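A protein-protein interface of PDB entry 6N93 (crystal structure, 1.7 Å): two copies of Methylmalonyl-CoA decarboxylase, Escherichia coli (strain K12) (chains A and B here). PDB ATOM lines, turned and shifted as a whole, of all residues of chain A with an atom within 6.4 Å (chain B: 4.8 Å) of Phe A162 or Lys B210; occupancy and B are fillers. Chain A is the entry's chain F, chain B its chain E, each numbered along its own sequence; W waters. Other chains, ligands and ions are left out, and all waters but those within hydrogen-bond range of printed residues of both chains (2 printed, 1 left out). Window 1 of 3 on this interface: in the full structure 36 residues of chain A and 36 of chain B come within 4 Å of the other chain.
No position is printed for both chains. Of the 13 pairs that touch across the chains among the printed residues, none has its exchanged pair printed and touching as well.
Met A131 touches none of the printed residues of chain B. Printed residues of chain B within 4 Å of Lys A158: Asp B119 (2.9 Å) and Leu B213 (3.7 Å). Of the printed residues of chain B, Glu A159 touches Leu B120. Leu A160 touches none of the printed residues of chain B. Of the printed residues of chain B, Phe A162 touches Pro B98 (3.8 Å), Asp B119 (3.9 Å), Ile B198 (3.8 Å), Lys B201 (3.7 Å) and Lys B210 (3.9 Å). Of the printed residues of chain B, Thr A163 touches Ile B198 (3.8 Å) and Lys B201 (3.3 Å). Of the printed residues of chain A, Lys B201 touches Val A134 (3.7 Å), Phe A162 (3.7 Å) and Thr A163 (3.3 Å). Printed residues of chain A within 4 Å of Ile B209: Ile A161. Of the printed residues of chain A, Lys B210 touches Phe A162. The nearest printed residue of chain B that does not touch Phe A162 is Ile B206 (4.01 Å).
Water W1 lies within hydrogen-bond range of OD1 of Asp B119 (2.5 Å) and NZ of Lys A158 (3.3 Å). Water W2 lies within hydrogen-bond range of the backbone carbonyl oxygen of Lys B210 (2.9 Å), the side-chain amino group of Lys A158 (2.9 Å) and the backbone NH of Arg B214 (3.3 Å).
CG2 of Val A134 touches CB of Lys B201, 3.7 Å away. CG1 of Ile B206 touches CG1 of Val A134 (3.6 Å). Lys A158 touches Leu B213. Ile B209 touches Ile A161. Phe A162 touches Pro B98 (CD2 to CG, 3.8 Å). Phe A162 touches Asp B119 (CE2 to CB, 3.9 Å). Ile B198 touches Phe A162 (CG1 to O, 3.8 Å). Lys B201 touches Phe A162. Thr A163 touches Ile B198. Thr A163 touches Lys B201.
O of Phe B95 sits at hydrogen-bond distance from NZ of Lys B210 (2.9 Å). The side-chain amino group (NZ) of Lys B210 sits at hydrogen-bond distance from the backbone carbonyl oxygen (O) of Lys B97. N of Ile B99 sits at hydrogen-bond distance from OD2 of Asp B119 (2.8 Å). NZ of Lys B210 lies within salt-bridge range of OD2 of Asp B119 (2.8 Å). The side-chain hydroxyl (OG1) of Thr A163 is in hydrogen-bond range of the backbone carbonyl oxygen (O) of Glu A159. The side-chain hydroxyl of Thr A163 lies close to the backbone NH of Ser A165 (3.1 Å).
Of the 11 printed residues of chain A, 6 touch a printed residue of chain B. Hydrophobic or aromatic side chains of chain A within 4 Å of the printed part of chain B: Val A134, Ile A161 and Phe A162. Hydrophobic or aromatic side chains of chain B that line the printed part of chain A: Pro B98, Leu B120, Ile B198, Ile B206, Ile B209 and Leu B213. Among the printed residues, Asp or Glu carboxylates within 4 Å of a Lys or Arg side-chain nitrogen of the other chain: Lys A158 with Asp B119.
The side-chain amino group of Lys A158 is in salt-bridge range of the side-chain carboxylate of Asp B119, at 2.9 Å.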
ATOM      1  N   MET A 131     -13.584 -41.958  -4.922  1.00  0.00           N
ATOM      2  CA  MET A 131     -13.243 -41.271  -6.191  1.00  0.00           C
ATOM      3  C   MET A 131     -11.754 -40.916  -6.101  1.00  0.00           C
ATOM      4  O   MET A 131     -11.413 -40.102  -5.235  1.00  0.00           O
ATOM      5  CB  MET A 131     -14.123 -40.020  -6.386  1.00  0.00           C
ATOM      6  CG  MET A 131     -14.043 -39.453  -7.769  1.00  0.00           C
ATOM      7  SD  MET A 131     -14.574 -40.671  -8.992  1.00  0.00           S
ATOM      8  CE  MET A 131     -13.857 -40.002 -10.490  1.00  0.00           C
ATOM      9  N   VAL A 134      -7.069 -37.880  -7.550  1.00  0.00           N
ATOM     10  CA  VAL A 134      -5.982 -37.113  -6.871  1.00  0.00           C
ATOM     11  C   VAL A 134      -4.906 -38.080  -6.317  1.00  0.00           C
ATOM     12  O   VAL A 134      -3.844 -37.607  -5.907  1.00  0.00           O
ATOM     13  CB  VAL A 134      -6.495 -36.144  -5.792  1.00  0.00           C
ATOM     14  CG1 VAL A 134      -7.523 -35.207  -6.357  1.00  0.00           C
ATOM     15  CG2 VAL A 134      -7.033 -36.822  -4.543  1.00  0.00           C
ATOM     16  N   VAL A 157     -19.087 -33.721  -2.237  1.00  0.00           N
ATOM     17  CA  VAL A 157     -18.343 -34.176  -3.432  1.00  0.00           C
ATOM     18  C   VAL A 157     -16.873 -33.759  -3.279  1.00  0.00           C
ATOM     19  O   VAL A 157     -15.951 -34.539  -3.611  1.00  0.00           O
ATOM     20  CB  VAL A 157     -19.004 -33.594  -4.696  1.00  0.00           C
ATOM     21  CG1 VAL A 157     -18.116 -33.762  -5.897  1.00  0.00           C
ATOM     22  CG2 VAL A 157     -20.369 -34.250  -4.896  1.00  0.00           C
ATOM     23  N   LYS A 158     -16.627 -32.538  -2.823  1.00  0.00           N
ATOM     24  CA  LYS A 158     -15.238 -32.082  -2.637  1.00  0.00           C
ATOM     25  C   LYS A 158     -14.503 -32.947  -1.609  1.00  0.00           C
ATOM     26  O   LYS A 158     -13.323 -33.213  -1.847  1.00  0.00           O
ATOM     27  CB  LYS A 158     -15.197 -30.584  -2.352  1.00  0.00           C
ATOM     28  CG  LYS A 158     -15.562 -29.739  -3.577  1.00  0.00           C
ATOM     29  CD  LYS A 158     -15.856 -28.291  -3.080  1.00  0.00           C
ATOM     30  CE  LYS A 158     -16.232 -27.299  -4.110  1.00  0.00           C
ATOM     31  NZ  LYS A 158     -16.101 -25.929  -3.571  1.00  0.00           N
ATOM     32  N   GLU A 159     -15.115 -33.278  -0.482  1.00  0.00           N
ATOM     33  CA  GLU A 159     -14.475 -34.205   0.491  1.00  0.00           C
ATOM     34  C   GLU A 159     -14.129 -35.517  -0.228  1.00  0.00           C
ATOM     35  O   GLU A 159     -12.965 -35.986  -0.096  1.00  0.00           O
ATOM     36  CB  GLU A 159     -15.364 -34.445   1.692  1.00  0.00           C
ATOM     37  CG  GLU A 159     -14.772 -35.435   2.691  1.00  0.00           C
ATOM     38  CD  GLU A 159     -15.714 -35.804   3.832  1.00  0.00           C
ATOM     39  OE1 GLU A 159     -16.780 -35.148   4.010  1.00  0.00           O
ATOM     40  OE2 GLU A 159     -15.421 -36.817   4.490  1.00  0.00           O
ATOM     41  N   LEU A 160     -15.075 -36.123  -0.951  1.00  0.00           N
ATOM     42  CA  LEU A 160     -14.800 -37.403  -1.641  1.00  0.00           C
ATOM     43  C   LEU A 160     -13.577 -37.281  -2.564  1.00  0.00           C
ATOM     44  O   LEU A 160     -12.686 -38.159  -2.540  1.00  0.00           O
ATOM     45  CB  LEU A 160     -16.021 -37.783  -2.478  1.00  0.00           C
ATOM     46  CG  LEU A 160     -17.187 -38.362  -1.698  1.00  0.00           C
ATOM     47  CD1 LEU A 160     -18.385 -38.509  -2.630  1.00  0.00           C
ATOM     48  CD2 LEU A 160     -16.798 -39.734  -1.141  1.00  0.00           C
ATOM     49  N   ILE A 161     -13.536 -36.234  -3.384  1.00  0.00           N
ATOM     50  CA  ILE A 161     -12.512 -36.095  -4.440  1.00  0.00           C
ATOM     51  C   ILE A 161     -11.203 -35.661  -3.803  1.00  0.00           C
ATOM     52  O   ILE A 161     -10.180 -36.255  -4.158  1.00  0.00           O
ATOM     53  CB  ILE A 161     -12.966 -35.158  -5.570  1.00  0.00           C
ATOM     54  CG1 ILE A 161     -14.191 -35.736  -6.268  1.00  0.00           C
ATOM     55  CG2 ILE A 161     -11.835 -34.951  -6.546  1.00  0.00           C
ATOM     56  CD1 ILE A 161     -14.818 -34.775  -7.224  1.00  0.00           C
ATOM     57  N   PHE A 162     -11.212 -34.691  -2.885  1.00  0.00           N
ATOM     58  CA  PHE A 162      -9.940 -34.183  -2.308  1.00  0.00           C
ATOM     59  C   PHE A 162      -9.280 -35.204  -1.371  1.00  0.00           C
ATOM     60  O   PHE A 162      -8.032 -35.239  -1.333  1.00  0.00           O
ATOM     61  CB  PHE A 162     -10.129 -32.841  -1.604  1.00  0.00           C
ATOM     62  CG  PHE A 162     -10.636 -31.717  -2.472  1.00  0.00           C
ATOM     63  CD1 PHE A 162     -10.627 -31.786  -3.848  1.00  0.00           C
ATOM     64  CD2 PHE A 162     -11.105 -30.565  -1.882  1.00  0.00           C
ATOM     65  CE1 PHE A 162     -11.103 -30.725  -4.608  1.00  0.00           C
ATOM     66  CE2 PHE A 162     -11.563 -29.496  -2.639  1.00  0.00           C
ATOM     67  CZ  PHE A 162     -11.596 -29.599  -4.004  1.00  0.00           C
ATOM     68  N   THR A 163     -10.038 -36.015  -0.645  1.00  0.00           N
ATOM     69  CA  THR A 163      -9.458 -37.053   0.249  1.00  0.00           C
ATOM     70  C   THR A 163      -9.228 -38.361  -0.485  1.00  0.00           C
ATOM     71  O   THR A 163      -8.359 -39.109  -0.044  1.00  0.00           O
ATOM     72  CB  THR A 163     -10.344 -37.329   1.488  1.00  0.00           C
ATOM     73  OG1 THR A 163     -11.529 -37.984   1.033  1.00  0.00           O
ATOM     74  CG2 THR A 163     -10.705 -36.087   2.275  1.00  0.00           C
ATOM     75  N   ALA A 164      -9.973 -38.674  -1.546  1.00  0.00           N
ATOM     76  CA  ALA A 164      -9.999 -40.015  -2.189  1.00  0.00           C
ATOM     77  C   ALA A 164     -10.287 -41.124  -1.165  1.00  0.00           C
ATOM     78  O   ALA A 164      -9.985 -42.281  -1.464  1.00  0.00           O
ATOM     79  CB  ALA A 164      -8.703 -40.277  -2.918  1.00  0.00           C
ATOM     80  N   SER A 165     -10.845 -40.822   0.001  1.00  0.00           N
ATOM     81  CA  SER A 165     -11.112 -41.841   1.053  1.00  0.00           C
ATOM     82  C   SER A 165     -12.431 -42.529   0.759  1.00  0.00           C
ATOM     83  O   SER A 165     -13.383 -41.893   0.300  1.00  0.00           O
ATOM     84  CB  SER A 165     -11.159 -41.247   2.445  1.00  0.00           C
ATOM     85  OG  SER A 165      -9.988 -40.534   2.746  1.00  0.00           O
ATOM     86  N   ILE B  92     -11.750 -17.261  -1.956  1.00  0.00           N
ATOM     87  CA  ILE B  92     -11.828 -18.636  -1.404  1.00  0.00           C
ATOM     88  C   ILE B  92     -12.125 -19.593  -2.553  1.00  0.00           C
ATOM     89  O   ILE B  92     -11.477 -20.619  -2.678  1.00  0.00           O
ATOM     90  CB  ILE B  92     -12.880 -18.690  -0.292  1.00  0.00           C
ATOM     91  CG1 ILE B  92     -12.380 -17.950   0.955  1.00  0.00           C
ATOM     92  CG2 ILE B  92     -13.282 -20.091   0.024  1.00  0.00           C
ATOM     93  CD1 ILE B  92     -13.417 -17.718   2.015  1.00  0.00           C
ATOM     94  N   GLN B  93     -13.096 -19.246  -3.396  1.00  0.00           N
ATOM     95  CA  GLN B  93     -13.563 -20.147  -4.484  1.00  0.00           C
ATOM     96  C   GLN B  93     -12.492 -20.316  -5.570  1.00  0.00           C
ATOM     97  O   GLN B  93     -12.387 -21.423  -6.080  1.00  0.00           O
ATOM     98  CB  GLN B  93     -14.875 -19.598  -5.035  1.00  0.00           C
ATOM     99  CG  GLN B  93     -16.054 -19.791  -4.101  1.00  0.00           C
ATOM    100  CD  GLN B  93     -17.282 -19.077  -4.595  1.00  0.00           C
ATOM    101  OE1 GLN B  93     -17.148 -18.085  -5.322  1.00  0.00           O
ATOM    102  NE2 GLN B  93     -18.465 -19.530  -4.151  1.00  0.00           N
ATOM    103  N   PHE B  95      -9.166 -20.065  -5.055  1.00  0.00           N
ATOM    104  CA  PHE B  95      -7.883 -20.426  -4.408  1.00  0.00           C
ATOM    105  C   PHE B  95      -7.543 -21.843  -4.816  1.00  0.00           C
ATOM    106  O   PHE B  95      -8.375 -22.758  -4.693  1.00  0.00           O
ATOM    107  CB  PHE B  95      -8.012 -20.180  -2.903  1.00  0.00           C
ATOM    108  CG  PHE B  95      -6.700 -20.074  -2.198  1.00  0.00           C
ATOM    109  CD1 PHE B  95      -5.930 -18.923  -2.332  1.00  0.00           C
ATOM    110  CD2 PHE B  95      -6.218 -21.145  -1.465  1.00  0.00           C
ATOM    111  CE1 PHE B  95      -4.708 -18.841  -1.683  1.00  0.00           C
ATOM    112  CE2 PHE B  95      -4.986 -21.064  -0.827  1.00  0.00           C
ATOM    113  CZ  PHE B  95      -4.235 -19.909  -0.950  1.00  0.00           C
ATOM    114  N   LYS B  97      -6.017 -24.291  -3.648  1.00  0.00           N
ATOM    115  CA  LYS B  97      -5.884 -25.305  -2.595  1.00  0.00           C
ATOM    116  C   LYS B  97      -7.219 -25.421  -1.904  1.00  0.00           C
ATOM    117  O   LYS B  97      -7.979 -24.473  -1.847  1.00  0.00           O
ATOM    118  CB  LYS B  97      -4.796 -24.888  -1.620  1.00  0.00           C
ATOM    119  CG  LYS B  97      -3.458 -24.581  -2.308  1.00  0.00           C
ATOM    120  CD  LYS B  97      -2.520 -23.843  -1.466  1.00  0.00           C
ATOM    121  CE  LYS B  97      -1.444 -23.131  -2.270  1.00  0.00           C
ATOM    122  NZ  LYS B  97      -0.572 -24.100  -2.977  1.00  0.00           N
ATOM    123  N   PRO B  98      -7.532 -26.586  -1.342  1.00  0.00           N
ATOM    124  CA  PRO B  98      -8.729 -26.725  -0.519  1.00  0.00           C
ATOM    125  C   PRO B  98      -8.689 -25.819   0.708  1.00  0.00           C
ATOM    126  O   PRO B  98      -7.624 -25.687   1.354  1.00  0.00           O
ATOM    127  CB  PRO B  98      -8.722 -28.189  -0.108  1.00  0.00           C
ATOM    128  CG  PRO B  98      -7.857 -28.817  -1.101  1.00  0.00           C
ATOM    129  CD  PRO B  98      -6.749 -27.820  -1.370  1.00  0.00           C
ATOM    130  N   ILE B  99      -9.845 -25.212   1.004  1.00  0.00           N
ATOM    131  CA  ILE B  99     -10.060 -24.361   2.194  1.00  0.00           C
ATOM    132  C   ILE B  99     -11.162 -25.028   3.022  1.00  0.00           C
ATOM    133  O   ILE B  99     -12.311 -25.174   2.526  1.00  0.00           O
ATOM    134  CB  ILE B  99     -10.365 -22.898   1.807  1.00  0.00           C
ATOM    135  CG1 ILE B  99      -9.184 -22.261   1.064  1.00  0.00           C
ATOM    136  CG2 ILE B  99     -10.703 -22.088   3.040  1.00  0.00           C
ATOM    137  CD1 ILE B  99      -9.489 -20.923   0.436  1.00  0.00           C
ATOM    138  N   ASP B 119     -14.620 -25.109   0.809  1.00  0.00           N
ATOM    139  CA  ASP B 119     -14.675 -26.432   0.137  1.00  0.00           C
ATOM    140  C   ASP B 119     -15.310 -27.480   1.056  1.00  0.00           C
ATOM    141  O   ASP B 119     -16.064 -28.356   0.548  1.00  0.00           O
ATOM    142  CB  ASP B 119     -13.299 -26.811  -0.355  1.00  0.00           C
ATOM    143  CG  ASP B 119     -12.782 -25.795  -1.371  1.00  0.00           C
ATOM    144  OD1 ASP B 119     -13.552 -25.473  -2.352  1.00  0.00           O
ATOM    145  OD2 ASP B 119     -11.682 -25.240  -1.120  1.00  0.00           O
ATOM    146  N   LEU B 120     -14.995 -27.457   2.360  1.00  0.00           N
ATOM    147  CA  LEU B 120     -15.520 -28.445   3.333  1.00  0.00           C
ATOM    148  C   LEU B 120     -15.794 -27.676   4.614  1.00  0.00           C
ATOM    149  O   LEU B 120     -15.110 -26.626   4.878  1.00  0.00           O
ATOM    150  CB  LEU B 120     -14.483 -29.535   3.670  1.00  0.00           C
ATOM    151  CG  LEU B 120     -14.201 -30.694   2.720  1.00  0.00           C
ATOM    152  CD1 LEU B 120     -13.316 -30.291   1.581  1.00  0.00           C
ATOM    153  CD2 LEU B 120     -13.501 -31.834   3.475  1.00  0.00           C
ATOM    154  N   ILE B 198      -5.245 -34.912   2.884  1.00  0.00           N
ATOM    155  CA  ILE B 198      -5.438 -34.198   1.592  1.00  0.00           C
ATOM    156  C   ILE B 198      -4.081 -33.739   1.064  1.00  0.00           C
ATOM    157  O   ILE B 198      -3.877 -33.861  -0.127  1.00  0.00           O
ATOM    158  CB  ILE B 198      -6.425 -33.048   1.776  1.00  0.00           C
ATOM    159  CG1 ILE B 198      -7.825 -33.588   2.048  1.00  0.00           C
ATOM    160  CG2 ILE B 198      -6.408 -32.091   0.624  1.00  0.00           C
ATOM    161  CD1 ILE B 198      -8.832 -32.581   2.516  1.00  0.00           C
ATOM    162  N   LYS B 201      -1.940 -35.776  -1.391  1.00  0.00           N
ATOM    163  CA  LYS B 201      -2.525 -36.041  -2.731  1.00  0.00           C
ATOM    164  C   LYS B 201      -1.958 -35.048  -3.738  1.00  0.00           C
ATOM    165  O   LYS B 201      -1.299 -34.094  -3.346  1.00  0.00           O
ATOM    166  CB  LYS B 201      -4.050 -35.918  -2.609  1.00  0.00           C
ATOM    167  CG  LYS B 201      -4.679 -36.791  -1.539  1.00  0.00           C
ATOM    168  CD  LYS B 201      -4.329 -38.272  -1.666  1.00  0.00           C
ATOM    169  CE  LYS B 201      -5.126 -39.155  -0.730  1.00  0.00           C
ATOM    170  NZ  LYS B 201      -4.764 -40.583  -0.906  1.00  0.00           N
ATOM    171  N   ALA B 205      -3.915 -31.772  -9.577  1.00  0.00           N
ATOM    172  CA  ALA B 205      -5.219 -32.435  -9.824  1.00  0.00           C
ATOM    173  C   ALA B 205      -6.277 -31.823  -8.903  1.00  0.00           C
ATOM    174  O   ALA B 205      -7.405 -31.517  -9.371  1.00  0.00           O
ATOM    175  CB  ALA B 205      -5.120 -33.935  -9.641  1.00  0.00           C
ATOM    176  N   ILE B 206      -5.960 -31.643  -7.618  1.00  0.00           N
ATOM    177  CA  ILE B 206      -6.905 -30.970  -6.682  1.00  0.00           C
ATOM    178  C   ILE B 206      -7.285 -29.592  -7.249  1.00  0.00           C
ATOM    179  O   ILE B 206      -8.486 -29.306  -7.289  1.00  0.00           O
ATOM    180  CB  ILE B 206      -6.309 -30.889  -5.263  1.00  0.00           C
ATOM    181  CG1 ILE B 206      -6.286 -32.300  -4.653  1.00  0.00           C
ATOM    182  CG2 ILE B 206      -7.062 -29.897  -4.396  1.00  0.00           C
ATOM    183  CD1 ILE B 206      -5.560 -32.414  -3.332  1.00  0.00           C
ATOM    184  N   ALA B 207      -6.307 -28.788  -7.677  1.00  0.00           N
ATOM    185  CA  ALA B 207      -6.565 -27.391  -8.113  1.00  0.00           C
ATOM    186  C   ALA B 207      -7.475 -27.399  -9.350  1.00  0.00           C
ATOM    187  O   ALA B 207      -8.440 -26.640  -9.390  1.00  0.00           O
ATOM    188  CB  ALA B 207      -5.267 -26.702  -8.409  1.00  0.00           C
ATOM    189  N   VAL B 208      -7.190 -28.244 -10.355  1.00  0.00           N
ATOM    190  CA  VAL B 208      -8.012 -28.193 -11.606  1.00  0.00           C
ATOM    191  C   VAL B 208      -9.422 -28.747 -11.317  1.00  0.00           C
ATOM    192  O   VAL B 208     -10.380 -28.174 -11.818  1.00  0.00           O
ATOM    193  CB  VAL B 208      -7.337 -28.837 -12.819  1.00  0.00           C
ATOM    194  CG1 VAL B 208      -7.242 -30.341 -12.720  1.00  0.00           C
ATOM    195  CG2 VAL B 208      -8.059 -28.427 -14.092  1.00  0.00           C
ATOM    196  N   ILE B 209      -9.572 -29.761 -10.482  1.00  0.00           N
ATOM    197  CA  ILE B 209     -10.930 -30.286 -10.178  1.00  0.00           C
ATOM    198  C   ILE B 209     -11.699 -29.268  -9.359  1.00  0.00           C
ATOM    199  O   ILE B 209     -12.870 -29.000  -9.690  1.00  0.00           O
ATOM    200  CB  ILE B 209     -10.813 -31.655  -9.495  1.00  0.00           C
ATOM    201  CG1 ILE B 209     -10.245 -32.685 -10.475  1.00  0.00           C
ATOM    202  CG2 ILE B 209     -12.177 -32.046  -8.947  1.00  0.00           C
ATOM    203  CD1 ILE B 209      -9.804 -34.024  -9.837  1.00  0.00           C
ATOM    204  N   LYS B 210     -11.020 -28.560  -8.446  1.00  0.00           N
ATOM    205  CA  LYS B 210     -11.675 -27.486  -7.682  1.00  0.00           C
ATOM    206  C   LYS B 210     -12.169 -26.438  -8.673  1.00  0.00           C
ATOM    207  O   LYS B 210     -13.314 -25.965  -8.503  1.00  0.00           O
ATOM    208  CB  LYS B 210     -10.779 -26.863  -6.612  1.00  0.00           C
ATOM    209  CG  LYS B 210     -11.407 -25.683  -5.914  1.00  0.00           C
ATOM    210  CD  LYS B 210     -10.662 -25.208  -4.694  1.00  0.00           C
ATOM    211  CE  LYS B 210     -11.143 -23.848  -4.253  1.00  0.00           C
ATOM    212  NZ  LYS B 210     -10.596 -23.483  -2.936  1.00  0.00           N
ATOM    213  N   GLU B 211     -11.329 -26.007  -9.629  1.00  0.00           N
ATOM    214  CA  GLU B 211     -11.734 -24.944 -10.572  1.00  0.00           C
ATOM    215  C   GLU B 211     -12.872 -25.446 -11.478  1.00  0.00           C
ATOM    216  O   GLU B 211     -13.742 -24.632 -11.865  1.00  0.00           O
ATOM    217  CB  GLU B 211     -10.522 -24.492 -11.383  1.00  0.00           C
ATOM    218  CG  GLU B 211     -10.845 -23.385 -12.376  1.00  0.00           C
ATOM    219  CD  GLU B 211     -11.255 -22.031 -11.832  1.00  0.00           C
ATOM    220  OE1 GLU B 211     -11.325 -21.813 -10.567  1.00  0.00           O
ATOM    221  OE2 GLU B 211     -11.489 -21.145 -12.670  1.00  0.00           O
ATOM    222  N   GLU B 212     -12.865 -26.720 -11.883  1.00  0.00           N
ATOM    223  CA  GLU B 212     -13.930 -27.300 -12.749  1.00  0.00           C
ATOM    224  C   GLU B 212     -15.262 -27.261 -11.973  1.00  0.00           C
ATOM    225  O   GLU B 212     -16.331 -26.809 -12.542  1.00  0.00           O
ATOM    226  CB  GLU B 212     -13.596 -28.733 -13.177  1.00  0.00           C
ATOM    227  CG  GLU B 212     -12.545 -28.811 -14.237  1.00  0.00           C
ATOM    228  CD  GLU B 212     -12.055 -30.230 -14.506  1.00  0.00           C
ATOM    229  OE1 GLU B 212     -12.186 -31.099 -13.658  1.00  0.00           O
ATOM    230  OE2 GLU B 212     -11.604 -30.461 -15.559  1.00  0.00           O
ATOM    231  N   LEU B 213     -15.235 -27.632 -10.690  1.00  0.00           N
ATOM    232  CA  LEU B 213     -16.433 -27.515  -9.824  1.00  0.00           C
ATOM    233  C   LEU B 213     -16.863 -26.055  -9.655  1.00  0.00           C
ATOM    234  O   LEU B 213     -18.083 -25.814  -9.706  1.00  0.00           O
ATOM    235  CB  LEU B 213     -16.181 -28.177  -8.474  1.00  0.00           C
ATOM    236  CG  LEU B 213     -16.147 -29.691  -8.494  1.00  0.00           C
ATOM    237  CD1 LEU B 213     -15.472 -30.227  -7.236  1.00  0.00           C
ATOM    238  CD2 LEU B 213     -17.553 -30.254  -8.642  1.00  0.00           C
ATOM    239  N   ARG B 214     -15.923 -25.126  -9.530  1.00  0.00           N
ATOM    240  CA  ARG B 214     -16.281 -23.685  -9.389  1.00  0.00           C
ATOM    241  C   ARG B 214     -17.036 -23.242 -10.642  1.00  0.00           C
ATOM    242  O   ARG B 214     -18.119 -22.618 -10.513  1.00  0.00           O
ATOM    243  CB  ARG B 214     -15.063 -22.798  -9.180  1.00  0.00           C
ATOM    244  CG  ARG B 214     -15.472 -21.362  -8.858  1.00  0.00           C
ATOM    245  CD  ARG B 214     -14.281 -20.438  -8.780  1.00  0.00           C
ATOM    246  NE  ARG B 214     -13.684 -20.223 -10.085  1.00  0.00           N
ATOM    247  CZ  ARG B 214     -14.139 -19.355 -10.995  1.00  0.00           C
ATOM    248  NH1 ARG B 214     -15.178 -18.573 -10.743  1.00  0.00           N
ATOM    249  NH2 ARG B 214     -13.492 -19.230 -12.137  1.00  0.00           N
HETATM  250  O   HOH W   1     -14.522 -23.183  -2.824  1.00  0.00           O
HETATM  251  O   HOH W   2     -15.189 -25.444  -6.326  1.00  0.00           O
